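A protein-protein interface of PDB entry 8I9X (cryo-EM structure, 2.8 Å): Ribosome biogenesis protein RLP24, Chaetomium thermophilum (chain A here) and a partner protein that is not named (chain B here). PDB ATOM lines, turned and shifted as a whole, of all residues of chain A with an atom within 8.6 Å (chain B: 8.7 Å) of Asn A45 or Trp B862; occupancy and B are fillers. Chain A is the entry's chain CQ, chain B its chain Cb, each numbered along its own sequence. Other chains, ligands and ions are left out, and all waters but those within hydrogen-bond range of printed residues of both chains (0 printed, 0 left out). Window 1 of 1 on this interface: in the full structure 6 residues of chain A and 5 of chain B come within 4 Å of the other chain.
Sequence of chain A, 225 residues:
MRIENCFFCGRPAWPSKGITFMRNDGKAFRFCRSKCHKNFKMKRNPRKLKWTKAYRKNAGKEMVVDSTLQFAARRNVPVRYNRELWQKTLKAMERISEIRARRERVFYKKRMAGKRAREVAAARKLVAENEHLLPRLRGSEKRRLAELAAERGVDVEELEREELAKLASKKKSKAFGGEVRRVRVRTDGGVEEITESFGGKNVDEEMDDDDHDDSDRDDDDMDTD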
ATOM      1  N   PHE A   7      12.817   4.434  18.463  1.00  0.00           N
ATOM      2  CA  PHE A   7      11.659   5.299  18.275  1.00  0.00           C
ATOM      3  C   PHE A   7      11.255   5.383  16.811  1.00  0.00           C
ATOM      4  O   PHE A   7      10.062   5.455  16.495  1.00  0.00           O
ATOM      5  CB  PHE A   7      11.955   6.695  18.817  1.00  0.00           C
ATOM      6  CG  PHE A   7      10.832   7.666  18.623  1.00  0.00           C
ATOM      7  CD1 PHE A   7       9.689   7.585  19.396  1.00  0.00           C
ATOM      8  CD2 PHE A   7      10.916   8.653  17.659  1.00  0.00           C
ATOM      9  CE1 PHE A   7       8.653   8.475  19.216  1.00  0.00           C
ATOM     10  CE2 PHE A   7       9.882   9.544  17.473  1.00  0.00           C
ATOM     11  CZ  PHE A   7       8.749   9.456  18.253  1.00  0.00           C
ATOM     12  N   PHE A   8      12.232   5.377  15.909  1.00  0.00           N
ATOM     13  CA  PHE A   8      11.952   5.648  14.506  1.00  0.00           C
ATOM     14  C   PHE A   8      11.523   4.391  13.760  1.00  0.00           C
ATOM     15  O   PHE A   8      10.473   4.374  13.110  1.00  0.00           O
ATOM     16  CB  PHE A   8      13.181   6.268  13.850  1.00  0.00           C
ATOM     17  CG  PHE A   8      12.861   7.147  12.692  1.00  0.00           C
ATOM     18  CD1 PHE A   8      12.341   8.412  12.892  1.00  0.00           C
ATOM     19  CD2 PHE A   8      13.076   6.712  11.403  1.00  0.00           C
ATOM     20  CE1 PHE A   8      12.046   9.227  11.823  1.00  0.00           C
ATOM     21  CE2 PHE A   8      12.784   7.520  10.336  1.00  0.00           C
ATOM     22  CZ  PHE A   8      12.267   8.780  10.542  1.00  0.00           C
ATOM     23  N   ASN A  39      17.510  10.661  10.014  1.00  0.00           N
ATOM     24  CA  ASN A  39      16.155  10.772   9.492  1.00  0.00           C
ATOM     25  C   ASN A  39      15.248  11.575  10.412  1.00  0.00           C
ATOM     26  O   ASN A  39      14.486  12.422   9.931  1.00  0.00           O
ATOM     27  CB  ASN A  39      15.560   9.383   9.260  1.00  0.00           C
ATOM     28  CG  ASN A  39      16.104   8.717   8.014  1.00  0.00           C
ATOM     29  OD1 ASN A  39      16.112   9.308   6.935  1.00  0.00           O
ATOM     30  ND2 ASN A  39      16.556   7.478   8.154  1.00  0.00           N
ATOM     31  N   PHE A  40      15.326  11.339  11.723  1.00  0.00           N
ATOM     32  CA  PHE A  40      14.536  12.124  12.665  1.00  0.00           C
ATOM     33  C   PHE A  40      14.941  13.592  12.632  1.00  0.00           C
ATOM     34  O   PHE A  40      14.082  14.480  12.699  1.00  0.00           O
ATOM     35  CB  PHE A  40      14.690  11.551  14.072  1.00  0.00           C
ATOM     36  CG  PHE A  40      13.923  12.298  15.123  1.00  0.00           C
ATOM     37  CD1 PHE A  40      12.590  12.014  15.356  1.00  0.00           C
ATOM     38  CD2 PHE A  40      14.535  13.282  15.879  1.00  0.00           C
ATOM     39  CE1 PHE A  40      11.883  12.695  16.322  1.00  0.00           C
ATOM     40  CE2 PHE A  40      13.831  13.968  16.845  1.00  0.00           C
ATOM     41  CZ  PHE A  40      12.504  13.674  17.067  1.00  0.00           C
ATOM     42  N   MET A  42      16.273  15.298  10.086  1.00  0.00           N
ATOM     43  CA  MET A  42      15.729  15.893   8.874  1.00  0.00           C
ATOM     44  C   MET A  42      14.214  15.778   8.823  1.00  0.00           C
ATOM     45  O   MET A  42      13.600  16.176   7.828  1.00  0.00           O
ATOM     46  CB  MET A  42      16.356  15.262   7.627  1.00  0.00           C
ATOM     47  CG  MET A  42      16.047  13.796   7.432  1.00  0.00           C
ATOM     48  SD  MET A  42      16.913  13.133   5.999  1.00  0.00           S
ATOM     49  CE  MET A  42      18.595  13.054   6.602  1.00  0.00           C
ATOM     50  N   LYS A  43      13.616  15.215   9.871  1.00  0.00           N
ATOM     51  CA  LYS A  43      12.188  15.334  10.152  1.00  0.00           C
ATOM     52  C   LYS A  43      11.354  14.659   9.072  1.00  0.00           C
ATOM     53  O   LYS A  43      10.446  15.246   8.480  1.00  0.00           O
ATOM     54  CB  LYS A  43      11.798  16.799  10.336  1.00  0.00           C
ATOM     55  CG  LYS A  43      12.414  17.404  11.586  1.00  0.00           C
ATOM     56  CD  LYS A  43      11.990  18.840  11.792  1.00  0.00           C
ATOM     57  CE  LYS A  43      12.683  19.431  13.003  1.00  0.00           C
ATOM     58  NZ  LYS A  43      12.224  18.782  14.264  1.00  0.00           N
ATOM     59  N   ARG A  44      11.678  13.399   8.823  1.00  0.00           N
ATOM     60  CA  ARG A  44      10.903  12.553   7.936  1.00  0.00           C
ATOM     61  C   ARG A  44       9.932  11.727   8.762  1.00  0.00           C
ATOM     62  O   ARG A  44      10.129  11.524   9.963  1.00  0.00           O
ATOM     63  CB  ARG A  44      11.821  11.639   7.128  1.00  0.00           C
ATOM     64  CG  ARG A  44      12.788  12.373   6.225  1.00  0.00           C
ATOM     65  CD  ARG A  44      13.818  11.422   5.652  1.00  0.00           C
ATOM     66  NE  ARG A  44      14.217  11.798   4.302  1.00  0.00           N
ATOM     67  CZ  ARG A  44      15.232  11.258   3.644  1.00  0.00           C
ATOM     68  NH1 ARG A  44      15.977  10.306   4.183  1.00  0.00           N
ATOM     69  NH2 ARG A  44      15.507  11.681   2.414  1.00  0.00           N
ATOM     70  N   ASN A  45       8.879  11.249   8.112  1.00  0.00           N
ATOM     71  CA  ASN A  45       7.857  10.482   8.810  1.00  0.00           C
ATOM     72  C   ASN A  45       8.197   8.998   8.761  1.00  0.00           C
ATOM     73  O   ASN A  45       8.280   8.427   7.661  1.00  0.00           O
ATOM     74  CB  ASN A  45       6.490  10.727   8.198  1.00  0.00           C
ATOM     75  CG  ASN A  45       5.365  10.524   9.190  1.00  0.00           C
ATOM     76  OD1 ASN A  45       5.528   9.835  10.196  1.00  0.00           O
ATOM     77  ND2 ASN A  45       4.216  11.125   8.914  1.00  0.00           N
ATOM     78  N   PRO A  46       8.419   8.346   9.904  1.00  0.00           N
ATOM     79  CA  PRO A  46       8.539   6.882   9.893  1.00  0.00           C
ATOM     80  C   PRO A  46       7.284   6.201   9.394  1.00  0.00           C
ATOM     81  O   PRO A  46       7.355   5.076   8.886  1.00  0.00           O
ATOM     82  CB  PRO A  46       8.821   6.544  11.364  1.00  0.00           C
ATOM     83  CG  PRO A  46       8.307   7.713  12.127  1.00  0.00           C
ATOM     84  CD  PRO A  46       8.561   8.901  11.259  1.00  0.00           C
ATOM     85  N   ARG A  47       6.130   6.853   9.531  1.00  0.00           N
ATOM     86  CA  ARG A  47       4.885   6.347   8.978  1.00  0.00           C
ATOM     87  C   ARG A  47       4.867   6.382   7.457  1.00  0.00           C
ATOM     88  O   ARG A  47       3.992   5.759   6.848  1.00  0.00           O
ATOM     89  CB  ARG A  47       3.713   7.155   9.541  1.00  0.00           C
ATOM     90  CG  ARG A  47       3.226   6.664  10.895  1.00  0.00           C
ATOM     91  CD  ARG A  47       1.906   5.931  10.784  1.00  0.00           C
ATOM     92  NE  ARG A  47       0.944   6.684   9.989  1.00  0.00           N
ATOM     93  CZ  ARG A  47       0.100   7.577  10.486  1.00  0.00           C
ATOM     94  NH1 ARG A  47       0.066   7.852  11.779  1.00  0.00           N
ATOM     95  NH2 ARG A  47      -0.732   8.211   9.665  1.00  0.00           N
ATOM     96  N   LYS A  48       5.809   7.093   6.836  1.00  0.00           N
ATOM     97  CA  LYS A  48       5.939   7.151   5.387  1.00  0.00           C
ATOM     98  C   LYS A  48       7.115   6.340   4.862  1.00  0.00           C
ATOM     99  O   LYS A  48       7.003   5.728   3.796  1.00  0.00           O
ATOM    100  CB  LYS A  48       6.076   8.603   4.922  1.00  0.00           C
ATOM    101  CG  LYS A  48       4.830   9.440   5.140  1.00  0.00           C
ATOM    102  CD  LYS A  48       5.015  10.849   4.608  1.00  0.00           C
ATOM    103  CE  LYS A  48       3.799  11.708   4.898  1.00  0.00           C
ATOM    104  NZ  LYS A  48       2.607  11.257   4.130  1.00  0.00           N
ATOM    105  N   LEU A  49       8.241   6.322   5.573  1.00  0.00           N
ATOM    106  CA  LEU A  49       9.348   5.469   5.156  1.00  0.00           C
ATOM    107  C   LEU A  49       8.974   4.000   5.303  1.00  0.00           C
ATOM    108  O   LEU A  49       8.558   3.551   6.373  1.00  0.00           O
ATOM    109  CB  LEU A  49      10.607   5.781   5.964  1.00  0.00           C
ATOM    110  CG  LEU A  49      10.992   7.252   6.044  1.00  0.00           C
ATOM    111  CD1 LEU A  49      12.070   7.463   7.068  1.00  0.00           C
ATOM    112  CD2 LEU A  49      11.487   7.687   4.692  1.00  0.00           C
ATOM    113  N   LYS A  50       9.153   3.246   4.220  1.00  0.00           N
ATOM    114  CA  LYS A  50       8.597   1.906   4.089  1.00  0.00           C
ATOM    115  C   LYS A  50       9.360   0.854   4.888  1.00  0.00           C
ATOM    116  O   LYS A  50       8.807  -0.215   5.164  1.00  0.00           O
ATOM    117  CB  LYS A  50       8.544   1.519   2.605  1.00  0.00           C
ATOM    118  CG  LYS A  50       7.922   0.162   2.305  1.00  0.00           C
ATOM    119  CD  LYS A  50       7.810  -0.077   0.809  1.00  0.00           C
ATOM    120  CE  LYS A  50       7.327  -1.484   0.511  1.00  0.00           C
ATOM    121  NZ  LYS A  50       5.933  -1.696   0.981  1.00  0.00           N
ATOM    122  N   TRP A  51      10.594   1.134   5.299  1.00  0.00           N
ATOM    123  CA  TRP A  51      11.391   0.180   6.054  1.00  0.00           C
ATOM    124  C   TRP A  51      11.198   0.312   7.558  1.00  0.00           C
ATOM    125  O   TRP A  51      12.094  -0.057   8.322  1.00  0.00           O
ATOM    126  CB  TRP A  51      12.874   0.335   5.712  1.00  0.00           C
ATOM    127  CG  TRP A  51      13.338   1.756   5.664  1.00  0.00           C
ATOM    128  CD1 TRP A  51      13.309   2.593   4.591  1.00  0.00           C
ATOM    129  CD2 TRP A  51      13.904   2.507   6.743  1.00  0.00           C
ATOM    130  NE1 TRP A  51      13.822   3.820   4.933  1.00  0.00           N
ATOM    131  CE2 TRP A  51      14.194   3.793   6.251  1.00  0.00           C
ATOM    132  CE3 TRP A  51      14.194   2.216   8.079  1.00  0.00           C
ATOM    133  CZ2 TRP A  51      14.758   4.786   7.045  1.00  0.00           C
ATOM    134  CZ3 TRP A  51      14.754   3.204   8.866  1.00  0.00           C
ATOM    135  CH2 TRP A  51      15.030   4.472   8.347  1.00  0.00           C
ATOM    136  N   THR A  52      10.054   0.821   8.001  1.00  0.00           N
ATOM    137  CA  THR A  52       9.796   1.047   9.414  1.00  0.00           C
ATOM    138  C   THR A  52       8.583   0.248   9.871  1.00  0.00           C
ATOM    139  O   THR A  52       7.633   0.027   9.111  1.00  0.00           O
ATOM    140  CB  THR A  52       9.569   2.533   9.702  1.00  0.00           C
ATOM    141  OG1 THR A  52       8.399   2.982   9.006  1.00  0.00           O
ATOM    142  CG2 THR A  52      10.763   3.351   9.244  1.00  0.00           C
ATOM    143  N   ALA A  54       6.419   1.290  11.905  1.00  0.00           N
ATOM    144  CA  ALA A  54       5.272   2.188  11.852  1.00  0.00           C
ATOM    145  C   ALA A  54       4.561   2.076  10.510  1.00  0.00           C
ATOM    146  O   ALA A  54       3.340   1.890  10.447  1.00  0.00           O
ATOM    147  CB  ALA A  54       5.722   3.626  12.112  1.00  0.00           C
ATOM    148  N   TYR A  55       5.326   2.160   9.419  1.00  0.00           N
ATOM    149  CA  TYR A  55       4.740   2.036   8.089  1.00  0.00           C
ATOM    150  C   TYR A  55       4.123   0.661   7.890  1.00  0.00           C
ATOM    151  O   TYR A  55       3.041   0.533   7.309  1.00  0.00           O
ATOM    152  CB  TYR A  55       5.797   2.301   7.016  1.00  0.00           C
ATOM    153  CG  TYR A  55       5.304   2.114   5.593  1.00  0.00           C
ATOM    154  CD1 TYR A  55       4.859   3.195   4.847  1.00  0.00           C
ATOM    155  CD2 TYR A  55       5.285   0.858   4.997  1.00  0.00           C
ATOM    156  CE1 TYR A  55       4.407   3.030   3.552  1.00  0.00           C
ATOM    157  CE2 TYR A  55       4.828   0.684   3.708  1.00  0.00           C
ATOM    158  CZ  TYR A  55       4.396   1.774   2.988  1.00  0.00           C
ATOM    159  OH  TYR A  55       3.946   1.607   1.698  1.00  0.00           O
ATOM    160  N   ASN A  58       0.919   0.383   9.768  1.00  0.00           N
ATOM    161  CA  ASN A  58      -0.101   1.217   9.141  1.00  0.00           C
ATOM    162  C   ASN A  58      -0.648   0.580   7.871  1.00  0.00           C
ATOM    163  O   ASN A  58      -1.858   0.626   7.627  1.00  0.00           O
ATOM    164  CB  ASN A  58       0.464   2.600   8.827  1.00  0.00           C
ATOM    165  CG  ASN A  58      -0.617   3.609   8.496  1.00  0.00           C
ATOM    166  OD1 ASN A  58      -1.808   3.302   8.553  1.00  0.00           O
ATOM    167  ND2 ASN A  58      -0.207   4.814   8.125  1.00  0.00           N
ATOM    168  N   ALA B 859      11.543  20.596  -0.230  1.00  0.00           N
ATOM    169  CA  ALA B 859      10.541  19.693   0.315  1.00  0.00           C
ATOM    170  C   ALA B 859      10.978  18.245   0.143  1.00  0.00           C
ATOM    171  O   ALA B 859      11.572  17.876  -0.873  1.00  0.00           O
ATOM    172  CB  ALA B 859       9.193  19.926  -0.367  1.00  0.00           C
ATOM    173  N   ASP B 860      10.686  17.427   1.149  1.00  0.00           N
ATOM    174  CA  ASP B 860      10.976  16.002   1.112  1.00  0.00           C
ATOM    175  C   ASP B 860       9.661  15.239   1.017  1.00  0.00           C
ATOM    176  O   ASP B 860       8.699  15.564   1.721  1.00  0.00           O
ATOM    177  CB  ASP B 860      11.759  15.573   2.354  1.00  0.00           C
ATOM    178  CG  ASP B 860      12.266  14.144   2.267  1.00  0.00           C
ATOM    179  OD1 ASP B 860      11.988  13.462   1.258  1.00  0.00           O
ATOM    180  OD2 ASP B 860      12.950  13.700   3.215  1.00  0.00           O
ATOM    181  N   LYS B 861       9.621  14.236   0.137  1.00  0.00           N
ATOM    182  CA  LYS B 861       8.407  13.443  -0.024  1.00  0.00           C
ATOM    183  C   LYS B 861       8.020  12.764   1.282  1.00  0.00           C
ATOM    184  O   LYS B 861       6.831  12.644   1.603  1.00  0.00           O
ATOM    185  CB  LYS B 861       8.602  12.402  -1.125  1.00  0.00           C
ATOM    186  CG  LYS B 861       9.128  12.960  -2.435  1.00  0.00           C
ATOM    187  CD  LYS B 861       9.471  11.840  -3.403  1.00  0.00           C
ATOM    188  CE  LYS B 861      10.047  12.381  -4.699  1.00  0.00           C
ATOM    189  NZ  LYS B 861      10.428  11.285  -5.633  1.00  0.00           N
ATOM    190  N   TRP B 862       9.013  12.316   2.051  1.00  0.00           N
ATOM    191  CA  TRP B 862       8.734  11.617   3.298  1.00  0.00           C
ATOM    192  C   TRP B 862       8.379  12.583   4.420  1.00  0.00           C
ATOM    193  O   TRP B 862       7.843  12.163   5.451  1.00  0.00           O
ATOM    194  CB  TRP B 862       9.935  10.758   3.675  1.00  0.00           C
ATOM    195  CG  TRP B 862      10.490   9.994   2.510  1.00  0.00           C
ATOM    196  CD1 TRP B 862      11.788   9.970   2.093  1.00  0.00           C
ATOM    197  CD2 TRP B 862       9.770   9.121   1.627  1.00  0.00           C
ATOM    198  NE1 TRP B 862      11.920   9.152   0.999  1.00  0.00           N
ATOM    199  CE2 TRP B 862      10.696   8.615   0.695  1.00  0.00           C
ATOM    200  CE3 TRP B 862       8.433   8.720   1.532  1.00  0.00           C
ATOM    201  CZ2 TRP B 862      10.330   7.734  -0.319  1.00  0.00           C
ATOM    202  CZ3 TRP B 862       8.071   7.846   0.524  1.00  0.00           C
ATOM    203  CH2 TRP B 862       9.016   7.362  -0.388  1.00  0.00           C
ATOM    204  N   ARG B 863       8.679  13.866   4.246  1.00  0.00           N
ATOM    205  CA  ARG B 863       8.233  14.870   5.201  1.00  0.00           C
ATOM    206  C   ARG B 863       6.720  15.034   5.108  1.00  0.00           C
ATOM    207  O   ARG B 863       6.128  14.874   4.038  1.00  0.00           O
ATOM    208  CB  ARG B 863       8.945  16.197   4.937  1.00  0.00           C
ATOM    209  CG  ARG B 863       8.711  17.257   5.991  1.00  0.00           C
ATOM    210  CD  ARG B 863       9.324  18.583   5.576  1.00  0.00           C
ATOM    211  NE  ARG B 863       9.203  19.587   6.625  1.00  0.00           N
ATOM    212  CZ  ARG B 863      10.131  19.832   7.540  1.00  0.00           C
ATOM    213  NH1 ARG B 863      11.273  19.165   7.561  1.00  0.00           N
ATOM    214  NH2 ARG B 863       9.906  20.767   8.457  1.00  0.00           N
ATOM    215  N   ASP B 864       6.094  15.347   6.245  1.00  0.00           N
ATOM    216  CA  ASP B 864       4.635  15.357   6.318  1.00  0.00           C
ATOM    217  C   ASP B 864       4.029  16.407   5.393  1.00  0.00           C
ATOM    218  O   ASP B 864       3.120  16.111   4.609  1.00  0.00           O
ATOM    219  CB  ASP B 864       4.188  15.593   7.761  1.00  0.00           C
ATOM    220  CG  ASP B 864       3.842  14.307   8.480  1.00  0.00           C
ATOM    221  OD1 ASP B 864       3.805  13.247   7.821  1.00  0.00           O
ATOM    222  OD2 ASP B 864       3.606  14.353   9.705  1.00  0.00           O
ATOM    223  N   ASP B 865       4.521  17.645   5.468  1.00  0.00           N
ATOM    224  CA  ASP B 865       3.903  18.771   4.765  1.00  0.00           C
ATOM    225  C   ASP B 865       4.584  18.982   3.412  1.00  0.00           C
ATOM    226  O   ASP B 865       4.962  20.091   3.028  1.00  0.00           O
ATOM    227  CB  ASP B 865       3.963  20.020   5.635  1.00  0.00           C
ATOM    228  CG  ASP B 865       5.342  20.261   6.216  1.00  0.00           C
ATOM    229  OD1 ASP B 865       6.333  19.780   5.631  1.00  0.00           O
ATOM    230  OD2 ASP B 865       5.436  20.935   7.264  1.00  0.00           O
ATOM    231  N   TYR B 866       4.690  17.889   2.655  1.00  0.00           N
ATOM    232  CA  TYR B 866       5.436  17.876   1.400  1.00  0.00           C
ATOM    233  C   TYR B 866       4.837  18.817   0.360  1.00  0.00           C
ATOM    234  O   TYR B 866       5.556  19.626  -0.233  1.00  0.00           O
ATOM    235  CB  TYR B 866       5.504  16.447   0.846  1.00  0.00           C
ATOM    236  CG  TYR B 866       5.956  16.364  -0.596  1.00  0.00           C
ATOM    237  CD1 TYR B 866       7.157  16.934  -1.002  1.00  0.00           C
ATOM    238  CD2 TYR B 866       5.186  15.714  -1.549  1.00  0.00           C
ATOM    239  CE1 TYR B 866       7.573  16.861  -2.316  1.00  0.00           C
ATOM    240  CE2 TYR B 866       5.596  15.635  -2.865  1.00  0.00           C
ATOM    241  CZ  TYR B 866       6.790  16.211  -3.243  1.00  0.00           C
ATOM    242  OH  TYR B 866       7.204  16.135  -4.553  1.00  0.00           O
ATOM    243  N   GLU B 867       3.525  18.724   0.127  1.00  0.00           N
ATOM    244  CA  GLU B 867       2.903  19.523  -0.925  1.00  0.00           C
ATOM    245  C   GLU B 867       2.979  21.013  -0.614  1.00  0.00           C
ATOM    246  O   GLU B 867       3.312  21.823  -1.490  1.00  0.00           O
ATOM    247  CB  GLU B 867       1.453  19.088  -1.125  1.00  0.00           C
ATOM    248  CG  GLU B 867       1.300  17.759  -1.845  1.00  0.00           C
ATOM    249  CD  GLU B 867       1.082  17.924  -3.336  1.00  0.00           C
ATOM    250  OE1 GLU B 867       0.373  18.873  -3.733  1.00  0.00           O
ATOM    251  OE2 GLU B 867       1.618  17.104  -4.111  1.00  0.00           O
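The guanidinium group (NH1) of Arg A44 is in hydrogen-bond range of the side-chain amide oxygen (OD1) of Asn A39 (2.9 Å).
The guanidinium group of Arg A44 lies close to the side-chain sulfur of Met A42 (3.5 Å).
The backbone NH (N) of Arg A47 lies close to the side-chain amide oxygen (OD1) of Asn A45 (3.1 Å).
OG1 of Thr A52 is in hydrogen-bond range of O of Leu A49 (2.7 Å).
The backbone NH (N) of Trp B862 sits close to the side-chain carboxylate (OD1) of Asp B860, at 3.3 Å.
OD1 of Asp B865 is in salt-bridge range of NE of Arg B863 (3.0 Å).
Printed residues of chain A that touch a printed residue of chain B: Met A42, Lys A43, Arg A44, Asn A45, Lys A48 and Leu A49.
Printed residues of chain B that touch a printed residue of chain A: Asp B860, Lys B861, Trp B862, Arg B863 and Asp B864.
Among the printed residues, 10 pairs touch across the chains.
Among the printed residues, Asp or Glu carboxylates within 4 Å of a Lys or Arg side-chain nitrogen of the other chain: Arg A44 with Asp B860 (2.5 Å).
Of chain B, only Trp B862 (3.0 Å) and Asp B864 (2.4 Å) come within 4 Å of Asn A45.
Of the printed residues of chain A, Trp B862 touches Arg A44, Asn A45, Lys A48 and Leu A49.
No residue of chain B comes within 4 Å of Pro A46.
Of the printed residues of chain A, Asp B860 touches Arg A44.
Of the printed residues of chain A, Arg B863 touches Met A42 and Lys A43.
Of the printed residues of chain B, Lys A43 touches Arg B863.
Ala B859 touches none of the printed residues of chain A.
The nearest printed residue of chain A that does not touch Lys B861 is Arg A44 (6.7 Å).
The guanidinium group of Arg A44 lies within salt-bridge range of the side-chain carboxylate of Asp B860 (2.5 Å).
The backbone carbonyl oxygen (O) of Trp B862 lies within hydrogen-bond range of the backbone NH (N) of Asn A45, at 3.0 Å.
The side-chain amide nitrogen (ND2) of Asn A45 is in hydrogen-bond range of the side-chain carboxylate (OD1) of Asp B864.
Among the printed residues, merely in contact across the chains: Lys A48 with Trp B862, Lys A48 with Asp B864, Leu A49 with Trp B862, Lys A43 with Arg B863, Arg A44 with Trp B862, Met A42 with Arg B863 and Lys A48 with Lys B861.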
